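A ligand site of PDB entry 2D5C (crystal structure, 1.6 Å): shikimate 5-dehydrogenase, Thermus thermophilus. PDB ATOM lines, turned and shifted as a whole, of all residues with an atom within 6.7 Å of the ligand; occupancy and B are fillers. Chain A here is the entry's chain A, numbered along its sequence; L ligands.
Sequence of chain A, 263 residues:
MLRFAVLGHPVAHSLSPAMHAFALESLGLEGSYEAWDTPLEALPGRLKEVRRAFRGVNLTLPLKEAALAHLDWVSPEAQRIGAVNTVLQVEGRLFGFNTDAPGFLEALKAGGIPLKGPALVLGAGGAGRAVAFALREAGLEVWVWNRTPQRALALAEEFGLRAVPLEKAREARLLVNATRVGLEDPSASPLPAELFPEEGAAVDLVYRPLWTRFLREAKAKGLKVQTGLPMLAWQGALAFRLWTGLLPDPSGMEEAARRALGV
OG of Ser 14 is in hydrogen-bond range of O3 of the ligand (2.5 Å).
OG of Ser 16 is in hydrogen-bond range of O3 of the ligand (2.6 Å).
OD1 of Asp 100 sits at hydrogen-bond distance from O1 of the ligand.
An oxygen (O4) of the ligand is in hydrogen-bond range of the side-chain hydroxyl (OH) of Tyr 207 (2.8 Å).
The side-chain amino group of Lys 64 is in hydrogen-bond range of an oxygen (O5) of the ligand, 2.9 Å away.
OE1 of Gln 235 sits at hydrogen-bond distance from O2 of the ligand.
The side-chain amide nitrogen (ND2) of Asn 85 lies within hydrogen-bond range of an oxygen (O1) of the ligand (3.0 Å).
O5 of the ligand lies within hydrogen-bond range of OG1 of Thr 60 (3.2 Å).
The side-chain amide nitrogen of Asn 58 lies close to an oxygen (O2) of the ligand.
The side-chain carboxylate of Asp 100 is in salt-bridge range of the side-chain amino group of Lys 64, 2.9 Å away.
The side-chain amide nitrogen (ND2) of Asn 85 sits at hydrogen-bond distance from the side-chain amide oxygen (OE1) of Gln 235 (2.8 Å).
The side-chain amide nitrogen of Gln 235 sits at hydrogen-bond distance from the backbone carbonyl oxygen of Leu 232.
The backbone carbonyl oxygen (O) of Gln 235 lies within hydrogen-bond range of the side-chain hydroxyl (OG1) of Thr 99 (2.8 Å).
O of Asn 85 lies within hydrogen-bond range of ND2 of Asn 58 (3.0 Å).
N of Leu 59 is in hydrogen-bond range of O of Asn 85.
OD1 of Asn 58 is in hydrogen-bond range of OH of Tyr 33.
OG1 of Thr 86 is in hydrogen-bond range of ND2 of Asn 58 (3.2 Å).
Merely in contact with the ligand: Val 6 (3.6 Å) and Leu 59 (3.7 Å).
Hydrophobic or aromatic side chains within 4 Å of the ligand: Val 6.
Within 4 Å of the ligand: Val 6, Ser 14, Ser 16, Asn 58, Leu 59, Thr 60, Lys 64, Asn 85, Asp 100, Tyr 207 and Gln 235.
The nearest printed residue that does not touch the ligand is Leu 232 (4.1 Å).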
ATOM      1  N   VAL A   6      -2.291 -28.085   4.186  1.00  0.00           N
ATOM      2  CA  VAL A   6      -3.370 -28.732   3.451  1.00  0.00           C
ATOM      3  C   VAL A   6      -2.626 -29.802   2.654  1.00  0.00           C
ATOM      4  O   VAL A   6      -1.681 -29.500   1.931  1.00  0.00           O
ATOM      5  CB  VAL A   6      -4.130 -27.781   2.484  1.00  0.00           C
ATOM      6  CG1 VAL A   6      -3.171 -27.168   1.454  1.00  0.00           C
ATOM      7  CG2 VAL A   6      -5.241 -28.554   1.774  1.00  0.00           C
ATOM      8  N   VAL A  11      -2.449 -29.548  -4.897  1.00  0.00           N
ATOM      9  CA  VAL A  11      -2.723 -28.573  -3.848  1.00  0.00           C
ATOM     10  C   VAL A  11      -1.979 -27.253  -4.041  1.00  0.00           C
ATOM     11  O   VAL A  11      -2.200 -26.301  -3.294  1.00  0.00           O
ATOM     12  CB  VAL A  11      -2.362 -29.137  -2.458  1.00  0.00           C
ATOM     13  CG1 VAL A  11      -3.293 -30.291  -2.114  1.00  0.00           C
ATOM     14  CG2 VAL A  11      -0.907 -29.594  -2.427  1.00  0.00           C
ATOM     15  N   HIS A  13      -2.532 -25.056  -5.973  1.00  0.00           N
ATOM     16  CA  HIS A  13      -3.521 -24.010  -6.234  1.00  0.00           C
ATOM     17  C   HIS A  13      -4.527 -23.788  -5.101  1.00  0.00           C
ATOM     18  O   HIS A  13      -5.485 -23.022  -5.252  1.00  0.00           O
ATOM     19  CB  HIS A  13      -4.304 -24.341  -7.512  1.00  0.00           C
ATOM     20  CG  HIS A  13      -3.656 -23.834  -8.765  1.00  0.00           C
ATOM     21  ND1 HIS A  13      -2.342 -24.110  -9.089  1.00  0.00           N
ATOM     22  CD2 HIS A  13      -4.144 -23.082  -9.771  1.00  0.00           C
ATOM     23  CE1 HIS A  13      -2.053 -23.543 -10.248  1.00  0.00           C
ATOM     24  NE2 HIS A  13      -3.137 -22.907 -10.681  1.00  0.00           N
ATOM     25  N   SER A  14      -4.339 -24.456  -3.959  1.00  0.00           N
ATOM     26  CA  SER A  14      -5.276 -24.290  -2.863  1.00  0.00           C
ATOM     27  C   SER A  14      -5.343 -22.856  -2.345  1.00  0.00           C
ATOM     28  O   SER A  14      -4.338 -22.151  -2.305  1.00  0.00           O
ATOM     29  CB  SER A  14      -4.913 -25.215  -1.705  1.00  0.00           C
ATOM     30  OG  SER A  14      -5.714 -24.929  -0.573  1.00  0.00           O
ATOM     31  N   LEU A  15      -6.541 -22.428  -1.960  1.00  0.00           N
ATOM     32  CA  LEU A  15      -6.754 -21.097  -1.398  1.00  0.00           C
ATOM     33  C   LEU A  15      -6.705 -21.129   0.138  1.00  0.00           C
ATOM     34  O   LEU A  15      -6.862 -20.093   0.803  1.00  0.00           O
ATOM     35  CB  LEU A  15      -8.114 -20.540  -1.841  1.00  0.00           C
ATOM     36  CG  LEU A  15      -8.279 -20.180  -3.324  1.00  0.00           C
ATOM     37  CD1 LEU A  15      -9.642 -19.533  -3.536  1.00  0.00           C
ATOM     38  CD2 LEU A  15      -7.179 -19.225  -3.747  1.00  0.00           C
ATOM     39  N   SER A  16      -6.502 -22.310   0.711  1.00  0.00           N
ATOM     40  CA  SER A  16      -6.444 -22.423   2.167  1.00  0.00           C
ATOM     41  C   SER A  16      -5.267 -21.662   2.764  1.00  0.00           C
ATOM     42  O   SER A  16      -5.428 -21.005   3.796  1.00  0.00           O
ATOM     43  CB  SER A  16      -6.373 -23.896   2.581  1.00  0.00           C
ATOM     44  OG  SER A  16      -7.642 -24.484   2.364  1.00  0.00           O
ATOM     45  N   PRO A  17      -4.085 -21.730   2.145  1.00  0.00           N
ATOM     46  CA  PRO A  17      -2.965 -21.001   2.721  1.00  0.00           C
ATOM     47  C   PRO A  17      -3.315 -19.526   2.919  1.00  0.00           C
ATOM     48  O   PRO A  17      -3.005 -18.934   3.954  1.00  0.00           O
ATOM     49  CB  PRO A  17      -1.846 -21.215   1.714  1.00  0.00           C
ATOM     50  CG  PRO A  17      -2.138 -22.597   1.208  1.00  0.00           C
ATOM     51  CD  PRO A  17      -3.638 -22.556   1.010  1.00  0.00           C
ATOM     52  N   MET A  19      -6.373 -18.157   3.187  1.00  0.00           N
ATOM     53  CA  MET A  19      -7.423 -17.985   4.185  1.00  0.00           C
ATOM     54  C   MET A  19      -6.888 -18.066   5.601  1.00  0.00           C
ATOM     55  O   MET A  19      -7.261 -17.268   6.462  1.00  0.00           O
ATOM     56  CB  MET A  19      -8.500 -19.058   4.050  1.00  0.00           C
ATOM     57  CG  MET A  19      -9.379 -18.967   2.830  1.00  0.00           C
ATOM     58  SD  MET A  19     -10.820 -20.026   3.053  1.00  0.00           S
ATOM     59  CE  MET A  19     -10.069 -21.670   3.010  1.00  0.00           C
ATOM     60  N   TYR A  33       0.780 -21.910   7.364  1.00  0.00           N
ATOM     61  CA  TYR A  33      -0.157 -22.851   6.755  1.00  0.00           C
ATOM     62  C   TYR A  33       0.335 -22.987   5.317  1.00  0.00           C
ATOM     63  O   TYR A  33       0.161 -22.067   4.500  1.00  0.00           O
ATOM     64  CB  TYR A  33      -1.578 -22.279   6.776  1.00  0.00           C
ATOM     65  CG  TYR A  33      -2.641 -23.251   6.299  1.00  0.00           C
ATOM     66  CD1 TYR A  33      -2.649 -23.708   4.986  1.00  0.00           C
ATOM     67  CD2 TYR A  33      -3.607 -23.749   7.184  1.00  0.00           C
ATOM     68  CE1 TYR A  33      -3.600 -24.648   4.552  1.00  0.00           C
ATOM     69  CE2 TYR A  33      -4.555 -24.695   6.771  1.00  0.00           C
ATOM     70  CZ  TYR A  33      -4.539 -25.137   5.451  1.00  0.00           C
ATOM     71  OH  TYR A  33      -5.458 -26.075   5.018  1.00  0.00           O
ATOM     72  N   VAL A  57      -3.914 -30.414  10.081  1.00  0.00           N
ATOM     73  CA  VAL A  57      -3.848 -30.311   8.636  1.00  0.00           C
ATOM     74  C   VAL A  57      -5.228 -30.538   8.070  1.00  0.00           C
ATOM     75  O   VAL A  57      -6.073 -31.165   8.724  1.00  0.00           O
ATOM     76  CB  VAL A  57      -2.912 -31.380   7.981  1.00  0.00           C
ATOM     77  CG1 VAL A  57      -1.484 -31.203   8.448  1.00  0.00           C
ATOM     78  CG2 VAL A  57      -3.442 -32.793   8.283  1.00  0.00           C
ATOM     79  N   ASN A  58      -5.459 -29.972   6.900  1.00  0.00           N
ATOM     80  CA  ASN A  58      -6.714 -30.171   6.178  1.00  0.00           C
ATOM     81  C   ASN A  58      -6.339 -31.222   5.143  1.00  0.00           C
ATOM     82  O   ASN A  58      -5.170 -31.327   4.753  1.00  0.00           O
ATOM     83  CB  ASN A  58      -7.171 -28.879   5.487  1.00  0.00           C
ATOM     84  CG  ASN A  58      -7.926 -27.965   6.419  1.00  0.00           C
ATOM     85  OD1 ASN A  58      -7.679 -26.756   6.457  1.00  0.00           O
ATOM     86  ND2 ASN A  58      -8.864 -28.539   7.178  1.00  0.00           N
ATOM     87  N   LEU A  59      -7.312 -32.039   4.741  1.00  0.00           N
ATOM     88  CA  LEU A  59      -7.069 -33.062   3.742  1.00  0.00           C
ATOM     89  C   LEU A  59      -7.974 -32.809   2.566  1.00  0.00           C
ATOM     90  O   LEU A  59      -9.147 -32.454   2.745  1.00  0.00           O
ATOM     91  CB  LEU A  59      -7.367 -34.463   4.306  1.00  0.00           C
ATOM     92  CG  LEU A  59      -6.587 -34.986   5.501  1.00  0.00           C
ATOM     93  CD1 LEU A  59      -7.021 -36.413   5.779  1.00  0.00           C
ATOM     94  CD2 LEU A  59      -5.082 -34.925   5.241  1.00  0.00           C
ATOM     95  N   THR A  60      -7.446 -32.988   1.363  1.00  0.00           N
ATOM     96  CA  THR A  60      -8.232 -32.796   0.156  1.00  0.00           C
ATOM     97  C   THR A  60      -7.978 -34.018  -0.735  1.00  0.00           C
ATOM     98  O   THR A  60      -7.298 -34.956  -0.312  1.00  0.00           O
ATOM     99  CB  THR A  60      -7.805 -31.467  -0.549  1.00  0.00           C
ATOM    100  OG1 THR A  60      -8.880 -30.989  -1.369  1.00  0.00           O
ATOM    101  CG2 THR A  60      -6.562 -31.679  -1.407  1.00  0.00           C
ATOM    102  N   LEU A  61      -8.504 -34.025  -1.953  1.00  0.00           N
ATOM    103  CA  LEU A  61      -8.307 -35.163  -2.861  1.00  0.00           C
ATOM    104  C   LEU A  61      -6.836 -35.526  -3.007  1.00  0.00           C
ATOM    105  O   LEU A  61      -5.966 -34.660  -3.032  1.00  0.00           O
ATOM    106  CB  LEU A  61      -8.824 -34.864  -4.265  1.00  0.00           C
ATOM    107  CG  LEU A  61     -10.318 -34.730  -4.531  1.00  0.00           C
ATOM    108  CD1 LEU A  61     -10.855 -33.451  -3.909  1.00  0.00           C
ATOM    109  CD2 LEU A  61     -10.529 -34.724  -6.037  1.00  0.00           C
ATOM    110  N   LYS A  64      -9.050 -37.957   1.503  1.00  0.00           N
ATOM    111  CA  LYS A  64     -10.107 -37.927   2.517  1.00  0.00           C
ATOM    112  C   LYS A  64     -10.689 -39.243   3.011  1.00  0.00           C
ATOM    113  O   LYS A  64     -11.037 -39.350   4.187  1.00  0.00           O
ATOM    114  CB  LYS A  64     -11.260 -37.021   2.068  1.00  0.00           C
ATOM    115  CG  LYS A  64     -10.898 -35.540   2.005  1.00  0.00           C
ATOM    116  CD  LYS A  64     -12.150 -34.724   1.757  1.00  0.00           C
ATOM    117  CE  LYS A  64     -11.873 -33.238   1.719  1.00  0.00           C
ATOM    118  NZ  LYS A  64     -13.093 -32.505   1.332  1.00  0.00           N
ATOM    119  N   ASN A  85     -11.766 -34.285   6.589  1.00  0.00           N
ATOM    120  CA  ASN A  85     -11.148 -33.143   5.917  1.00  0.00           C
ATOM    121  C   ASN A  85     -10.293 -32.331   6.901  1.00  0.00           C
ATOM    122  O   ASN A  85      -9.570 -31.416   6.509  1.00  0.00           O
ATOM    123  CB  ASN A  85     -12.227 -32.245   5.304  1.00  0.00           C
ATOM    124  CG  ASN A  85     -12.762 -31.215   6.281  1.00  0.00           C
ATOM    125  OD1 ASN A  85     -13.154 -31.542   7.401  1.00  0.00           O
ATOM    126  ND2 ASN A  85     -12.797 -29.954   5.856  1.00  0.00           N
ATOM    127  N   THR A  86     -10.380 -32.680   8.177  1.00  0.00           N
ATOM    128  CA  THR A  86      -9.613 -31.970   9.194  1.00  0.00           C
ATOM    129  C   THR A  86      -9.011 -32.941  10.205  1.00  0.00           C
ATOM    130  O   THR A  86      -9.718 -33.771  10.778  1.00  0.00           O
ATOM    131  CB  THR A  86     -10.502 -30.957   9.950  1.00  0.00           C
ATOM    132  OG1 THR A  86     -11.062 -30.025   9.021  1.00  0.00           O
ATOM    133  CG2 THR A  86      -9.684 -30.199  11.002  1.00  0.00           C
ATOM    134  N   THR A  99     -15.265 -30.944   8.735  1.00  0.00           N
ATOM    135  CA  THR A  99     -15.881 -29.629   8.844  1.00  0.00           C
ATOM    136  C   THR A  99     -16.593 -29.228   7.555  1.00  0.00           C
ATOM    137  O   THR A  99     -17.205 -28.172   7.512  1.00  0.00           O
ATOM    138  CB  THR A  99     -14.848 -28.551   9.232  1.00  0.00           C
ATOM    139  OG1 THR A  99     -13.876 -28.404   8.188  1.00  0.00           O
ATOM    140  CG2 THR A  99     -14.144 -28.949  10.541  1.00  0.00           C
ATOM    141  N   ASP A 100     -16.539 -30.073   6.520  1.00  0.00           N
ATOM    142  CA  ASP A 100     -17.249 -29.773   5.255  1.00  0.00           C
ATOM    143  C   ASP A 100     -18.746 -29.761   5.521  1.00  0.00           C
ATOM    144  O   ASP A 100     -19.467 -28.906   5.009  1.00  0.00           O
ATOM    145  CB  ASP A 100     -16.961 -30.817   4.166  1.00  0.00           C
ATOM    146  CG  ASP A 100     -15.573 -30.704   3.574  1.00  0.00           C
ATOM    147  OD1 ASP A 100     -15.122 -29.576   3.249  1.00  0.00           O
ATOM    148  OD2 ASP A 100     -14.917 -31.761   3.421  1.00  0.00           O
ATOM    149  N   TYR A 207     -14.907 -24.141  -7.236  1.00  0.00           N
ATOM    150  CA  TYR A 207     -14.700 -22.699  -7.259  1.00  0.00           C
ATOM    151  C   TYR A 207     -13.551 -22.279  -8.201  1.00  0.00           C
ATOM    152  O   TYR A 207     -13.044 -21.160  -8.115  1.00  0.00           O
ATOM    153  CB  TYR A 207     -14.473 -22.153  -5.844  1.00  0.00           C
ATOM    154  CG  TYR A 207     -13.355 -22.818  -5.082  1.00  0.00           C
ATOM    155  CD1 TYR A 207     -12.018 -22.525  -5.375  1.00  0.00           C
ATOM    156  CD2 TYR A 207     -13.628 -23.746  -4.081  1.00  0.00           C
ATOM    157  CE1 TYR A 207     -10.979 -23.156  -4.687  1.00  0.00           C
ATOM    158  CE2 TYR A 207     -12.597 -24.377  -3.397  1.00  0.00           C
ATOM    159  CZ  TYR A 207     -11.288 -24.083  -3.701  1.00  0.00           C
ATOM    160  OH  TYR A 207     -10.275 -24.723  -3.027  1.00  0.00           O
ATOM    161  N   MET A 231     -18.599 -21.876   1.497  1.00  0.00           N
ATOM    162  CA  MET A 231     -18.379 -23.166   2.164  1.00  0.00           C
ATOM    163  C   MET A 231     -16.889 -23.357   2.442  1.00  0.00           C
ATOM    164  O   MET A 231     -16.507 -23.863   3.500  1.00  0.00           O
ATOM    165  CB  MET A 231     -18.868 -24.325   1.285  1.00  0.00           C
ATOM    166  CG  MET A 231     -18.706 -25.700   1.935  1.00  0.00           C
ATOM    167  SD  MET A 231     -19.355 -27.025   0.883  1.00  0.00           S
ATOM    168  CE  MET A 231     -18.688 -28.498   1.696  1.00  0.00           C
ATOM    169  N   LEU A 232     -16.041 -22.959   1.500  1.00  0.00           N
ATOM    170  CA  LEU A 232     -14.601 -23.107   1.684  1.00  0.00           C
ATOM    171  C   LEU A 232     -14.161 -22.346   2.938  1.00  0.00           C
ATOM    172  O   LEU A 232     -13.385 -22.854   3.755  1.00  0.00           O
ATOM    173  CB  LEU A 232     -13.855 -22.575   0.454  1.00  0.00           C
ATOM    174  CG  LEU A 232     -12.326 -22.692   0.492  1.00  0.00           C
ATOM    175  CD1 LEU A 232     -11.917 -24.140   0.585  1.00  0.00           C
ATOM    176  CD2 LEU A 232     -11.728 -22.060  -0.773  1.00  0.00           C
ATOM    177  N   GLN A 235     -15.790 -24.075   6.302  1.00  0.00           N
ATOM    178  CA  GLN A 235     -15.174 -25.324   6.721  1.00  0.00           C
ATOM    179  C   GLN A 235     -13.774 -25.025   7.262  1.00  0.00           C
ATOM    180  O   GLN A 235     -13.299 -25.693   8.190  1.00  0.00           O
ATOM    181  CB  GLN A 235     -15.128 -26.345   5.568  1.00  0.00           C
ATOM    182  CG  GLN A 235     -14.226 -26.016   4.376  1.00  0.00           C
ATOM    183  CD  GLN A 235     -12.743 -26.235   4.643  1.00  0.00           C
ATOM    184  OE1 GLN A 235     -12.353 -27.218   5.287  1.00  0.00           O
ATOM    185  NE2 GLN A 235     -11.906 -25.334   4.122  1.00  0.00           N
ATOM    186  N   GLY A 236     -13.134 -23.986   6.699  1.00  0.00           N
ATOM    187  CA  GLY A 236     -11.806 -23.606   7.150  1.00  0.00           C
ATOM    188  C   GLY A 236     -11.838 -22.966   8.541  1.00  0.00           C
ATOM    189  O   GLY A 236     -11.022 -23.313   9.394  1.00  0.00           O
ATOM    190  N   ALA A 239     -12.382 -25.545  11.088  1.00  0.00           N
ATOM    191  CA  ALA A 239     -11.208 -26.395  11.317  1.00  0.00           C
ATOM    192  C   ALA A 239     -10.228 -25.651  12.226  1.00  0.00           C
ATOM    193  O   ALA A 239      -9.617 -26.239  13.109  1.00  0.00           O
ATOM    194  CB  ALA A 239     -10.526 -26.752   9.992  1.00  0.00           C
HETATM  195  O1  LIG L   1     -12.405 -29.798   2.904  1.00  0.00           O
HETATM  196  C1  LIG L   1     -11.609 -28.784   2.270  1.00  0.00           C
HETATM  197  C2  LIG L   1     -10.138 -28.905   2.733  1.00  0.00           C
HETATM  198  O2  LIG L   1     -10.084 -28.765   4.148  1.00  0.00           O
HETATM  199  C3  LIG L   1      -9.248 -27.822   2.079  1.00  0.00           C
HETATM  200  C4  LIG L   1      -9.603 -27.561   0.614  1.00  0.00           C
HETATM  201  C5  LIG L   1      -8.681 -26.706  -0.182  1.00  0.00           C
HETATM  202  O3  LIG L   1      -7.566 -26.210   0.405  1.00  0.00           O
HETATM  203  O4  LIG L   1      -8.912 -26.453  -1.355  1.00  0.00           O
HETATM  204  C6  LIG L   1     -10.692 -28.051   0.017  1.00  0.00           C
HETATM  205  C7  LIG L   1     -11.708 -28.931   0.722  1.00  0.00           C
HETATM  206  O5  LIG L   1     -11.452 -30.304   0.354  1.00  0.00           O
